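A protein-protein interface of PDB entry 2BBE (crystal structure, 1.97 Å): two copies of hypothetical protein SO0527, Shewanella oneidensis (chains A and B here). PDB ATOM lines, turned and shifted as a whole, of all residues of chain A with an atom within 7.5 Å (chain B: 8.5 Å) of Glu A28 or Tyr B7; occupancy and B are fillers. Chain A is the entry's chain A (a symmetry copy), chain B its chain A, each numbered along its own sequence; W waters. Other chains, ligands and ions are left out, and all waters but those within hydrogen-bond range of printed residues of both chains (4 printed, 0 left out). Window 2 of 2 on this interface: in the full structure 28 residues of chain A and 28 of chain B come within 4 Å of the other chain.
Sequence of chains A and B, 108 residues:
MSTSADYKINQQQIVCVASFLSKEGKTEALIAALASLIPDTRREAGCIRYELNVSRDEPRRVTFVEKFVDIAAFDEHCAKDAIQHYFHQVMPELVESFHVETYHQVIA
OE1 of Glu A28 is in hydrogen-bond range of OH of Tyr B7 (2.8 Å).
The backbone NH (N) of Val B106 is in hydrogen-bond range of the backbone carbonyl oxygen (O) of Leu A52 (2.7 Å).
Water W2 bridges the side-chain carboxylate (OE1) of Glu A28 and the side-chain hydroxyl (OH) of Tyr B7.
Water W3 lies within hydrogen-bond range of O of Val B106 (2.5 Å), N of Leu A52 (2.9 Å) and NE2 of Gln B105 (3.1 Å).
Water W1 bridges the backbone carbonyl oxygen of Ala A32 (2.6 Å) and the side-chain carboxylate of Asp B6 (3.1 Å).
Water W4 bridges the side-chain hydroxyl of Tyr B7 (2.6 Å) and the backbone carbonyl oxygen of Glu A28 (2.9 Å).
The backbone NH (N) of Asn B10 is in hydrogen-bond range of the backbone carbonyl oxygen (O) of Gln B105 (2.8 Å).
No position is printed for both chains.
Printed residues of chain B that touch a printed residue of chain A: Tyr B7, Ile B9, Gln B105, Val B106 and Ala B108.
Printed residues of chain A that touch a printed residue of chain B: Glu A28, Ile A31, Ala A35, Leu A52 and Val A54.
Hydrophobic or aromatic side chains of chain A that line the printed part of chain B: Ile A31, Leu A52 and Val A54.
Among the printed residues, 7 pairs touch across the chains.
No residue of chain B comes within 4 Å of Thr A27.
Of the printed residues of chain B, Glu A28 touches Tyr B7 (2.8 Å).
Ala A29 touches none of the printed residues of chain B.
Printed residues of chain B within 4 Å of Ala A35: Ala B108 (3.9 Å).
Asp B6 touches none of the printed residues of chain A.
Of the printed residues of chain A, Tyr B7 touches Glu A28 and Ile A31.
Printed residues of chain A within 4 Å of Gln B105: Leu A52 (3.3 Å).
Of the printed residues of chain A, Val B106 touches Leu A52 (2.7 Å) and Val A54 (3.6 Å).
The nearest printed residue of chain B that does not touch Glu A28 is Ile B9 (6.0 Å).
The nearest printed residue of chain A that does not touch Ala B108 is Ile A38 (4.04 Å).
Among the printed residues, merely in contact across the chains: Ile A31 with Tyr B7 (3.4 Å), Ala A35 with Ala B108 (3.9 Å), Leu A52 with Gln B105 (3.3 Å), Val A54 with Ile B9 (3.96 Å) and Val A54 with Val B106 (3.6 Å).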
ATOM      1  N   SER A  22     -17.224  20.017 -35.156  1.00  0.00           N
ATOM      2  CA  SER A  22     -17.428  21.331 -35.759  1.00  0.00           C
ATOM      3  C   SER A  22     -17.616  21.212 -37.284  1.00  0.00           C
ATOM      4  O   SER A  22     -17.173  20.240 -37.919  1.00  0.00           O
ATOM      5  CB  SER A  22     -16.285  22.303 -35.436  1.00  0.00           C
ATOM      6  OG  SER A  22     -15.199  22.070 -36.305  1.00  0.00           O
ATOM      7  N   LYS A  23     -18.305  22.194 -37.852  1.00  0.00           N
ATOM      8  CA  LYS A  23     -18.282  22.401 -39.304  1.00  0.00           C
ATOM      9  C   LYS A  23     -16.869  22.829 -39.740  1.00  0.00           C
ATOM     10  O   LYS A  23     -16.066  23.276 -38.904  1.00  0.00           O
ATOM     11  CB  LYS A  23     -19.301  23.483 -39.691  1.00  0.00           C
ATOM     12  CG  LYS A  23     -20.753  23.114 -39.336  1.00  0.00           C
ATOM     13  CD  LYS A  23     -21.724  24.272 -39.590  1.00  0.00           C
ATOM     14  CE  LYS A  23     -23.195  23.782 -39.454  1.00  0.00           C
ATOM     15  NZ  LYS A  23     -24.192  24.562 -40.290  1.00  0.00           N
ATOM     16  N   GLY A  25     -13.945  24.962 -40.792  1.00  0.00           N
ATOM     17  CA  GLY A  25     -13.611  26.344 -40.478  1.00  0.00           C
ATOM     18  C   GLY A  25     -14.195  26.896 -39.186  1.00  0.00           C
ATOM     19  O   GLY A  25     -14.001  28.078 -38.876  1.00  0.00           O
ATOM     20  N   LYS A  26     -14.891  26.060 -38.419  1.00  0.00           N
ATOM     21  CA  LYS A  26     -15.568  26.535 -37.207  1.00  0.00           C
ATOM     22  C   LYS A  26     -14.964  25.975 -35.920  1.00  0.00           C
ATOM     23  O   LYS A  26     -15.523  26.180 -34.845  1.00  0.00           O
ATOM     24  CB  LYS A  26     -17.060  26.178 -37.248  1.00  0.00           C
ATOM     25  CG  LYS A  26     -17.849  26.801 -38.406  1.00  0.00           C
ATOM     26  CD  LYS A  26     -17.910  28.335 -38.295  1.00  0.00           C
ATOM     27  CE  LYS A  26     -18.827  28.945 -39.354  1.00  0.00           C
ATOM     28  NZ  LYS A  26     -18.925  30.456 -39.218  1.00  0.00           N
ATOM     29  N   THR A  27     -13.839  25.269 -36.022  1.00  0.00           N
ATOM     30  CA  THR A  27     -13.300  24.568 -34.850  1.00  0.00           C
ATOM     31  C   THR A  27     -12.854  25.538 -33.749  1.00  0.00           C
ATOM     32  O   THR A  27     -13.221  25.351 -32.595  1.00  0.00           O
ATOM     33  CB  THR A  27     -12.153  23.631 -35.225  1.00  0.00           C
ATOM     34  OG1 THR A  27     -12.580  22.765 -36.279  1.00  0.00           O
ATOM     35  CG2 THR A  27     -11.738  22.798 -34.017  1.00  0.00           C
ATOM     36  N   GLU A  28     -12.068  26.568 -34.091  1.00  0.00           N
ATOM     37  CA  GLU A  28     -11.645  27.551 -33.084  1.00  0.00           C
ATOM     38  C   GLU A  28     -12.832  28.251 -32.419  1.00  0.00           C
ATOM     39  O   GLU A  28     -12.853  28.418 -31.198  1.00  0.00           O
ATOM     40  CB  GLU A  28     -10.691  28.577 -33.690  1.00  0.00           C
ATOM     41  CG  GLU A  28      -9.392  27.952 -34.165  1.00  0.00           C
ATOM     42  CD  GLU A  28      -8.578  27.362 -33.029  1.00  0.00           C
ATOM     43  OE1 GLU A  28      -8.624  27.906 -31.900  1.00  0.00           O
ATOM     44  OE2 GLU A  28      -7.887  26.350 -33.264  1.00  0.00           O
ATOM     45  N   ALA A  29     -13.823  28.646 -33.223  1.00  0.00           N
ATOM     46  CA  ALA A  29     -15.077  29.231 -32.693  1.00  0.00           C
ATOM     47  C   ALA A  29     -15.802  28.253 -31.746  1.00  0.00           C
ATOM     48  O   ALA A  29     -16.328  28.659 -30.710  1.00  0.00           O
ATOM     49  CB  ALA A  29     -16.003  29.669 -33.834  1.00  0.00           C
ATOM     50  N   LEU A  30     -15.800  26.968 -32.092  1.00  0.00           N
ATOM     51  CA  LEU A  30     -16.462  25.978 -31.238  1.00  0.00           C
ATOM     52  C   LEU A  30     -15.738  25.803 -29.901  1.00  0.00           C
ATOM     53  O   LEU A  30     -16.384  25.765 -28.855  1.00  0.00           O
ATOM     54  CB  LEU A  30     -16.593  24.635 -31.946  1.00  0.00           C
ATOM     55  CG  LEU A  30     -17.274  23.542 -31.099  1.00  0.00           C
ATOM     56  CD1 LEU A  30     -18.730  23.969 -30.698  1.00  0.00           C
ATOM     57  CD2 LEU A  30     -17.243  22.211 -31.813  1.00  0.00           C
ATOM     58  N   ILE A  31     -14.407  25.693 -29.941  1.00  0.00           N
ATOM     59  CA  ILE A  31     -13.627  25.550 -28.698  1.00  0.00           C
ATOM     60  C   ILE A  31     -13.914  26.766 -27.811  1.00  0.00           C
ATOM     61  O   ILE A  31     -14.161  26.611 -26.622  1.00  0.00           O
ATOM     62  CB  ILE A  31     -12.078  25.417 -28.942  1.00  0.00           C
ATOM     63  CG1 ILE A  31     -11.742  24.179 -29.807  1.00  0.00           C
ATOM     64  CG2 ILE A  31     -11.294  25.366 -27.592  1.00  0.00           C
ATOM     65  CD1 ILE A  31     -10.315  24.202 -30.433  1.00  0.00           C
ATOM     66  N   ALA A  32     -13.870  27.964 -28.390  1.00  0.00           N
ATOM     67  CA  ALA A  32     -14.154  29.188 -27.628  1.00  0.00           C
ATOM     68  C   ALA A  32     -15.550  29.209 -26.985  1.00  0.00           C
ATOM     69  O   ALA A  32     -15.688  29.584 -25.808  1.00  0.00           O
ATOM     70  CB  ALA A  32     -13.927  30.436 -28.487  1.00  0.00           C
ATOM     71  N   ALA A  33     -16.562  28.794 -27.750  1.00  0.00           N
ATOM     72  CA  ALA A  33     -17.956  28.767 -27.298  1.00  0.00           C
ATOM     73  C   ALA A  33     -18.121  27.793 -26.129  1.00  0.00           C
ATOM     74  O   ALA A  33     -18.775  28.113 -25.116  1.00  0.00           O
ATOM     75  CB  ALA A  33     -18.888  28.379 -28.452  1.00  0.00           C
ATOM     76  N   LEU A  34     -17.519  26.610 -26.263  1.00  0.00           N
ATOM     77  CA  LEU A  34     -17.584  25.597 -25.182  1.00  0.00           C
ATOM     78  C   LEU A  34     -16.759  26.050 -23.967  1.00  0.00           C
ATOM     79  O   LEU A  34     -17.177  25.873 -22.818  1.00  0.00           O
ATOM     80  CB  LEU A  34     -17.113  24.224 -25.695  1.00  0.00           C
ATOM     81  CG  LEU A  34     -18.087  23.568 -26.708  1.00  0.00           C
ATOM     82  CD1 LEU A  34     -17.414  22.413 -27.434  1.00  0.00           C
ATOM     83  CD2 LEU A  34     -19.385  23.078 -26.024  1.00  0.00           C
ATOM     84  N   ALA A  35     -15.577  26.620 -24.213  1.00  0.00           N
ATOM     85  CA  ALA A  35     -14.730  27.032 -23.087  1.00  0.00           C
ATOM     86  C   ALA A  35     -15.397  28.134 -22.277  1.00  0.00           C
ATOM     87  O   ALA A  35     -15.159  28.241 -21.056  1.00  0.00           O
ATOM     88  CB  ALA A  35     -13.333  27.466 -23.557  1.00  0.00           C
ATOM     89  N   SER A  36     -16.219  28.954 -22.941  1.00  0.00           N
ATOM     90  CA  SER A  36     -16.903  30.064 -22.260  1.00  0.00           C
ATOM     91  C   SER A  36     -17.879  29.554 -21.175  1.00  0.00           C
ATOM     92  O   SER A  36     -18.227  30.301 -20.239  1.00  0.00           O
ATOM     93  CB  SER A  36     -17.651  30.962 -23.270  1.00  0.00           C
ATOM     94  OG  SER A  36     -18.836  30.290 -23.687  1.00  0.00           O
ATOM     95  N   ILE A  38     -17.252  27.096 -19.074  1.00  0.00           N
ATOM     96  CA  ILE A  38     -16.548  26.412 -17.982  1.00  0.00           C
ATOM     97  C   ILE A  38     -16.559  27.157 -16.621  1.00  0.00           C
ATOM     98  O   ILE A  38     -16.876  26.540 -15.593  1.00  0.00           O
ATOM     99  CB  ILE A  38     -15.105  25.995 -18.413  1.00  0.00           C
ATOM    100  CG1 ILE A  38     -15.203  24.935 -19.517  1.00  0.00           C
ATOM    101  CG2 ILE A  38     -14.290  25.455 -17.197  1.00  0.00           C
ATOM    102  CD1 ILE A  38     -13.852  24.510 -20.090  1.00  0.00           C
ATOM    103  N   LEU A  52     -12.905  20.215 -20.754  1.00  0.00           N
ATOM    104  CA  LEU A  52     -12.978  20.331 -22.213  1.00  0.00           C
ATOM    105  C   LEU A  52     -11.722  19.733 -22.872  1.00  0.00           C
ATOM    106  O   LEU A  52     -10.618  19.821 -22.324  1.00  0.00           O
ATOM    107  CB  LEU A  52     -13.139  21.813 -22.602  1.00  0.00           C
ATOM    108  CG  LEU A  52     -13.487  22.136 -24.065  1.00  0.00           C
ATOM    109  CD1 LEU A  52     -14.809  21.441 -24.514  1.00  0.00           C
ATOM    110  CD2 LEU A  52     -13.564  23.665 -24.242  1.00  0.00           C
ATOM    111  N   VAL A  54      -9.798  18.588 -26.865  1.00  0.00           N
ATOM    112  CA  VAL A  54      -9.745  18.639 -28.328  1.00  0.00           C
ATOM    113  C   VAL A  54      -9.111  17.358 -28.857  1.00  0.00           C
ATOM    114  O   VAL A  54      -8.056  16.909 -28.363  1.00  0.00           O
ATOM    115  CB  VAL A  54      -8.983  19.903 -28.857  1.00  0.00           C
ATOM    116  CG1 VAL A  54      -9.825  21.129 -28.583  1.00  0.00           C
ATOM    117  CG2 VAL A  54      -7.586  20.058 -28.188  1.00  0.00           C
ATOM    118  N   PRO A  59      -9.396  16.547 -35.627  1.00  0.00           N
ATOM    119  CA  PRO A  59      -9.215  17.841 -34.974  1.00  0.00           C
ATOM    120  C   PRO A  59     -10.437  18.790 -34.998  1.00  0.00           C
ATOM    121  O   PRO A  59     -10.407  19.782 -34.281  1.00  0.00           O
ATOM    122  CB  PRO A  59      -7.993  18.421 -35.684  1.00  0.00           C
ATOM    123  CG  PRO A  59      -7.292  17.194 -36.279  1.00  0.00           C
ATOM    124  CD  PRO A  59      -8.480  16.386 -36.768  1.00  0.00           C
ATOM    125  N   VAL A  62     -14.519  18.385 -30.509  1.00  0.00           N
ATOM    126  CA  VAL A  62     -14.277  18.982 -29.200  1.00  0.00           C
ATOM    127  C   VAL A  62     -15.257  18.299 -28.225  1.00  0.00           C
ATOM    128  O   VAL A  62     -16.453  18.191 -28.540  1.00  0.00           O
ATOM    129  CB  VAL A  62     -14.523  20.514 -29.241  1.00  0.00           C
ATOM    130  CG1 VAL A  62     -13.983  21.174 -27.988  1.00  0.00           C
ATOM    131  CG2 VAL A  62     -13.833  21.154 -30.486  1.00  0.00           C
ATOM    132  N   LEU A  94     -22.203  26.340 -35.552  1.00  0.00           N
ATOM    133  CA  LEU A  94     -20.833  25.824 -35.478  1.00  0.00           C
ATOM    134  C   LEU A  94     -20.666  24.322 -35.653  1.00  0.00           C
ATOM    135  O   LEU A  94     -19.559  23.860 -35.959  1.00  0.00           O
ATOM    136  CB  LEU A  94     -20.213  26.204 -34.116  1.00  0.00           C
ATOM    137  CG  LEU A  94     -20.209  27.686 -33.729  1.00  0.00           C
ATOM    138  CD1 LEU A  94     -19.367  27.919 -32.485  1.00  0.00           C
ATOM    139  CD2 LEU A  94     -19.671  28.546 -34.865  1.00  0.00           C
ATOM    140  N   ASP B   6      -7.824  33.376 -23.284  1.00  0.00           N
ATOM    141  CA  ASP B   6      -9.032  32.792 -22.627  1.00  0.00           C
ATOM    142  C   ASP B   6      -8.943  31.286 -22.326  1.00  0.00           C
ATOM    143  O   ASP B   6      -9.578  30.816 -21.364  1.00  0.00           O
ATOM    144  CB  ASP B   6     -10.319  33.101 -23.412  1.00  0.00           C
ATOM    145  CG  ASP B   6     -10.258  32.675 -24.896  1.00  0.00           C
ATOM    146  OD1 ASP B   6      -9.139  32.516 -25.449  1.00  0.00           O
ATOM    147  OD2 ASP B   6     -11.352  32.531 -25.518  1.00  0.00           O
ATOM    148  N   TYR B   7      -8.207  30.538 -23.150  1.00  0.00           N
ATOM    149  CA  TYR B   7      -7.958  29.108 -22.888  1.00  0.00           C
ATOM    150  C   TYR B   7      -6.574  28.691 -23.385  1.00  0.00           C
ATOM    151  O   TYR B   7      -5.997  29.343 -24.258  1.00  0.00           O
ATOM    152  CB  TYR B   7      -9.056  28.199 -23.496  1.00  0.00           C
ATOM    153  CG  TYR B   7      -9.081  28.136 -25.007  1.00  0.00           C
ATOM    154  CD1 TYR B   7      -8.161  27.345 -25.712  1.00  0.00           C
ATOM    155  CD2 TYR B   7     -10.020  28.866 -25.740  1.00  0.00           C
ATOM    156  CE1 TYR B   7      -8.172  27.291 -27.100  1.00  0.00           C
ATOM    157  CE2 TYR B   7     -10.035  28.813 -27.129  1.00  0.00           C
ATOM    158  CZ  TYR B   7      -9.102  28.018 -27.798  1.00  0.00           C
ATOM    159  OH  TYR B   7      -9.107  27.956 -29.176  1.00  0.00           O
ATOM    160  N   LYS B   8      -6.047  27.606 -22.832  1.00  0.00           N
ATOM    161  CA  LYS B   8      -4.786  27.046 -23.300  1.00  0.00           C
ATOM    162  C   LYS B   8      -4.908  25.526 -23.376  1.00  0.00           C
ATOM    163  O   LYS B   8      -5.310  24.881 -22.399  1.00  0.00           O
ATOM    164  CB  LYS B   8      -3.628  27.435 -22.374  1.00  0.00           C
ATOM    165  CG  LYS B   8      -2.284  26.789 -22.752  1.00  0.00           C
ATOM    166  CD  LYS B   8      -1.130  27.371 -21.952  1.00  0.00           C
ATOM    167  CE  LYS B   8       0.202  26.779 -22.376  1.00  0.00           C
ATOM    168  NZ  LYS B   8       1.363  27.433 -21.679  1.00  0.00           N
ATOM    169  N   ILE B   9      -4.541  24.973 -24.532  1.00  0.00           N
ATOM    170  CA  ILE B   9      -4.488  23.522 -24.711  1.00  0.00           C
ATOM    171  C   ILE B   9      -3.242  22.971 -23.983  1.00  0.00           C
ATOM    172  O   ILE B   9      -2.133  23.469 -24.168  1.00  0.00           O
ATOM    173  CB  ILE B   9      -4.486  23.142 -26.215  1.00  0.00           C
ATOM    174  CG1 ILE B   9      -5.744  23.694 -26.919  1.00  0.00           C
ATOM    175  CG2 ILE B   9      -4.409  21.594 -26.388  1.00  0.00           C
ATOM    176  CD1 ILE B   9      -5.729  23.556 -28.454  1.00  0.00           C
ATOM    177  N   ASN B  10      -3.435  21.970 -23.134  1.00  0.00           N
ATOM    178  CA  ASN B  10      -2.312  21.260 -22.526  1.00  0.00           C
ATOM    179  C   ASN B  10      -1.782  20.272 -23.565  1.00  0.00           C
ATOM    180  O   ASN B  10      -2.467  19.306 -23.927  1.00  0.00           O
ATOM    181  CB  ASN B  10      -2.767  20.548 -21.241  1.00  0.00           C
ATOM    182  CG  ASN B  10      -1.642  19.814 -20.525  1.00  0.00           C
ATOM    183  OD1 ASN B  10      -0.781  19.195 -21.136  1.00  0.00           O
ATOM    184  ND2 ASN B  10      -1.691  19.835 -19.205  1.00  0.00           N
ATOM    185  N   GLN B 105      -6.339  18.217 -23.259  1.00  0.00           N
ATOM    186  CA  GLN B 105      -7.275  18.968 -22.450  1.00  0.00           C
ATOM    187  C   GLN B 105      -7.135  20.448 -22.735  1.00  0.00           C
ATOM    188  O   GLN B 105      -6.024  20.939 -22.950  1.00  0.00           O
ATOM    189  CB  GLN B 105      -7.085  18.672 -20.958  1.00  0.00           C
ATOM    190  CG  GLN B 105      -8.232  19.227 -20.078  1.00  0.00           C
ATOM    191  CD  GLN B 105      -8.030  18.972 -18.578  1.00  0.00           C
ATOM    192  OE1 GLN B 105      -7.041  18.364 -18.159  1.00  0.00           O
ATOM    193  NE2 GLN B 105      -8.954  19.454 -17.776  1.00  0.00           N
ATOM    194  N   VAL B 106      -8.278  21.133 -22.775  1.00  0.00           N
ATOM    195  CA  VAL B 106      -8.360  22.596 -22.896  1.00  0.00           C
ATOM    196  C   VAL B 106      -8.644  23.201 -21.509  1.00  0.00           C
ATOM    197  O   VAL B 106      -9.698  22.937 -20.908  1.00  0.00           O
ATOM    198  CB  VAL B 106      -9.504  23.034 -23.863  1.00  0.00           C
ATOM    199  CG1 VAL B 106      -9.571  24.597 -23.995  1.00  0.00           C
ATOM    200  CG2 VAL B 106      -9.349  22.366 -25.210  1.00  0.00           C
ATOM    201  N   ILE B 107      -7.712  24.017 -21.030  1.00  0.00           N
ATOM    202  CA  ILE B 107      -7.827  24.681 -19.737  1.00  0.00           C
ATOM    203  C   ILE B 107      -8.372  26.094 -19.919  1.00  0.00           C
ATOM    204  O   ILE B 107      -7.770  26.909 -20.623  1.00  0.00           O
ATOM    205  CB  ILE B 107      -6.440  24.722 -19.007  1.00  0.00           C
ATOM    206  CG1 ILE B 107      -5.839  23.293 -18.902  1.00  0.00           C
ATOM    207  CG2 ILE B 107      -6.570  25.358 -17.612  1.00  0.00           C
ATOM    208  CD1 ILE B 107      -6.625  22.348 -17.922  1.00  0.00           C
ATOM    209  N   ALA B 108      -9.520  26.363 -19.304  1.00  0.00           N
ATOM    210  CA  ALA B 108     -10.102  27.698 -19.248  1.00  0.00           C
ATOM    211  C   ALA B 108     -10.396  28.071 -17.785  1.00  0.00           C
ATOM    212  O   ALA B 108     -10.641  27.181 -16.940  1.00  0.00           O
ATOM    213  CB  ALA B 108     -11.396  27.736 -20.057  1.00  0.00           C
ATOM    214  OXT ALA B 108     -10.429  29.259 -17.401  1.00  0.00           O
HETATM  215  O   HOH W   1     -14.072  31.350 -24.783  1.00  0.00           O
HETATM  216  O   HOH W   2      -7.239  26.303 -30.538  1.00  0.00           O
HETATM  217  O   HOH W   3     -10.851  21.530 -19.131  1.00  0.00           O
HETATM  218  O   HOH W   4     -10.555  29.933 -30.183  1.00  0.00           O
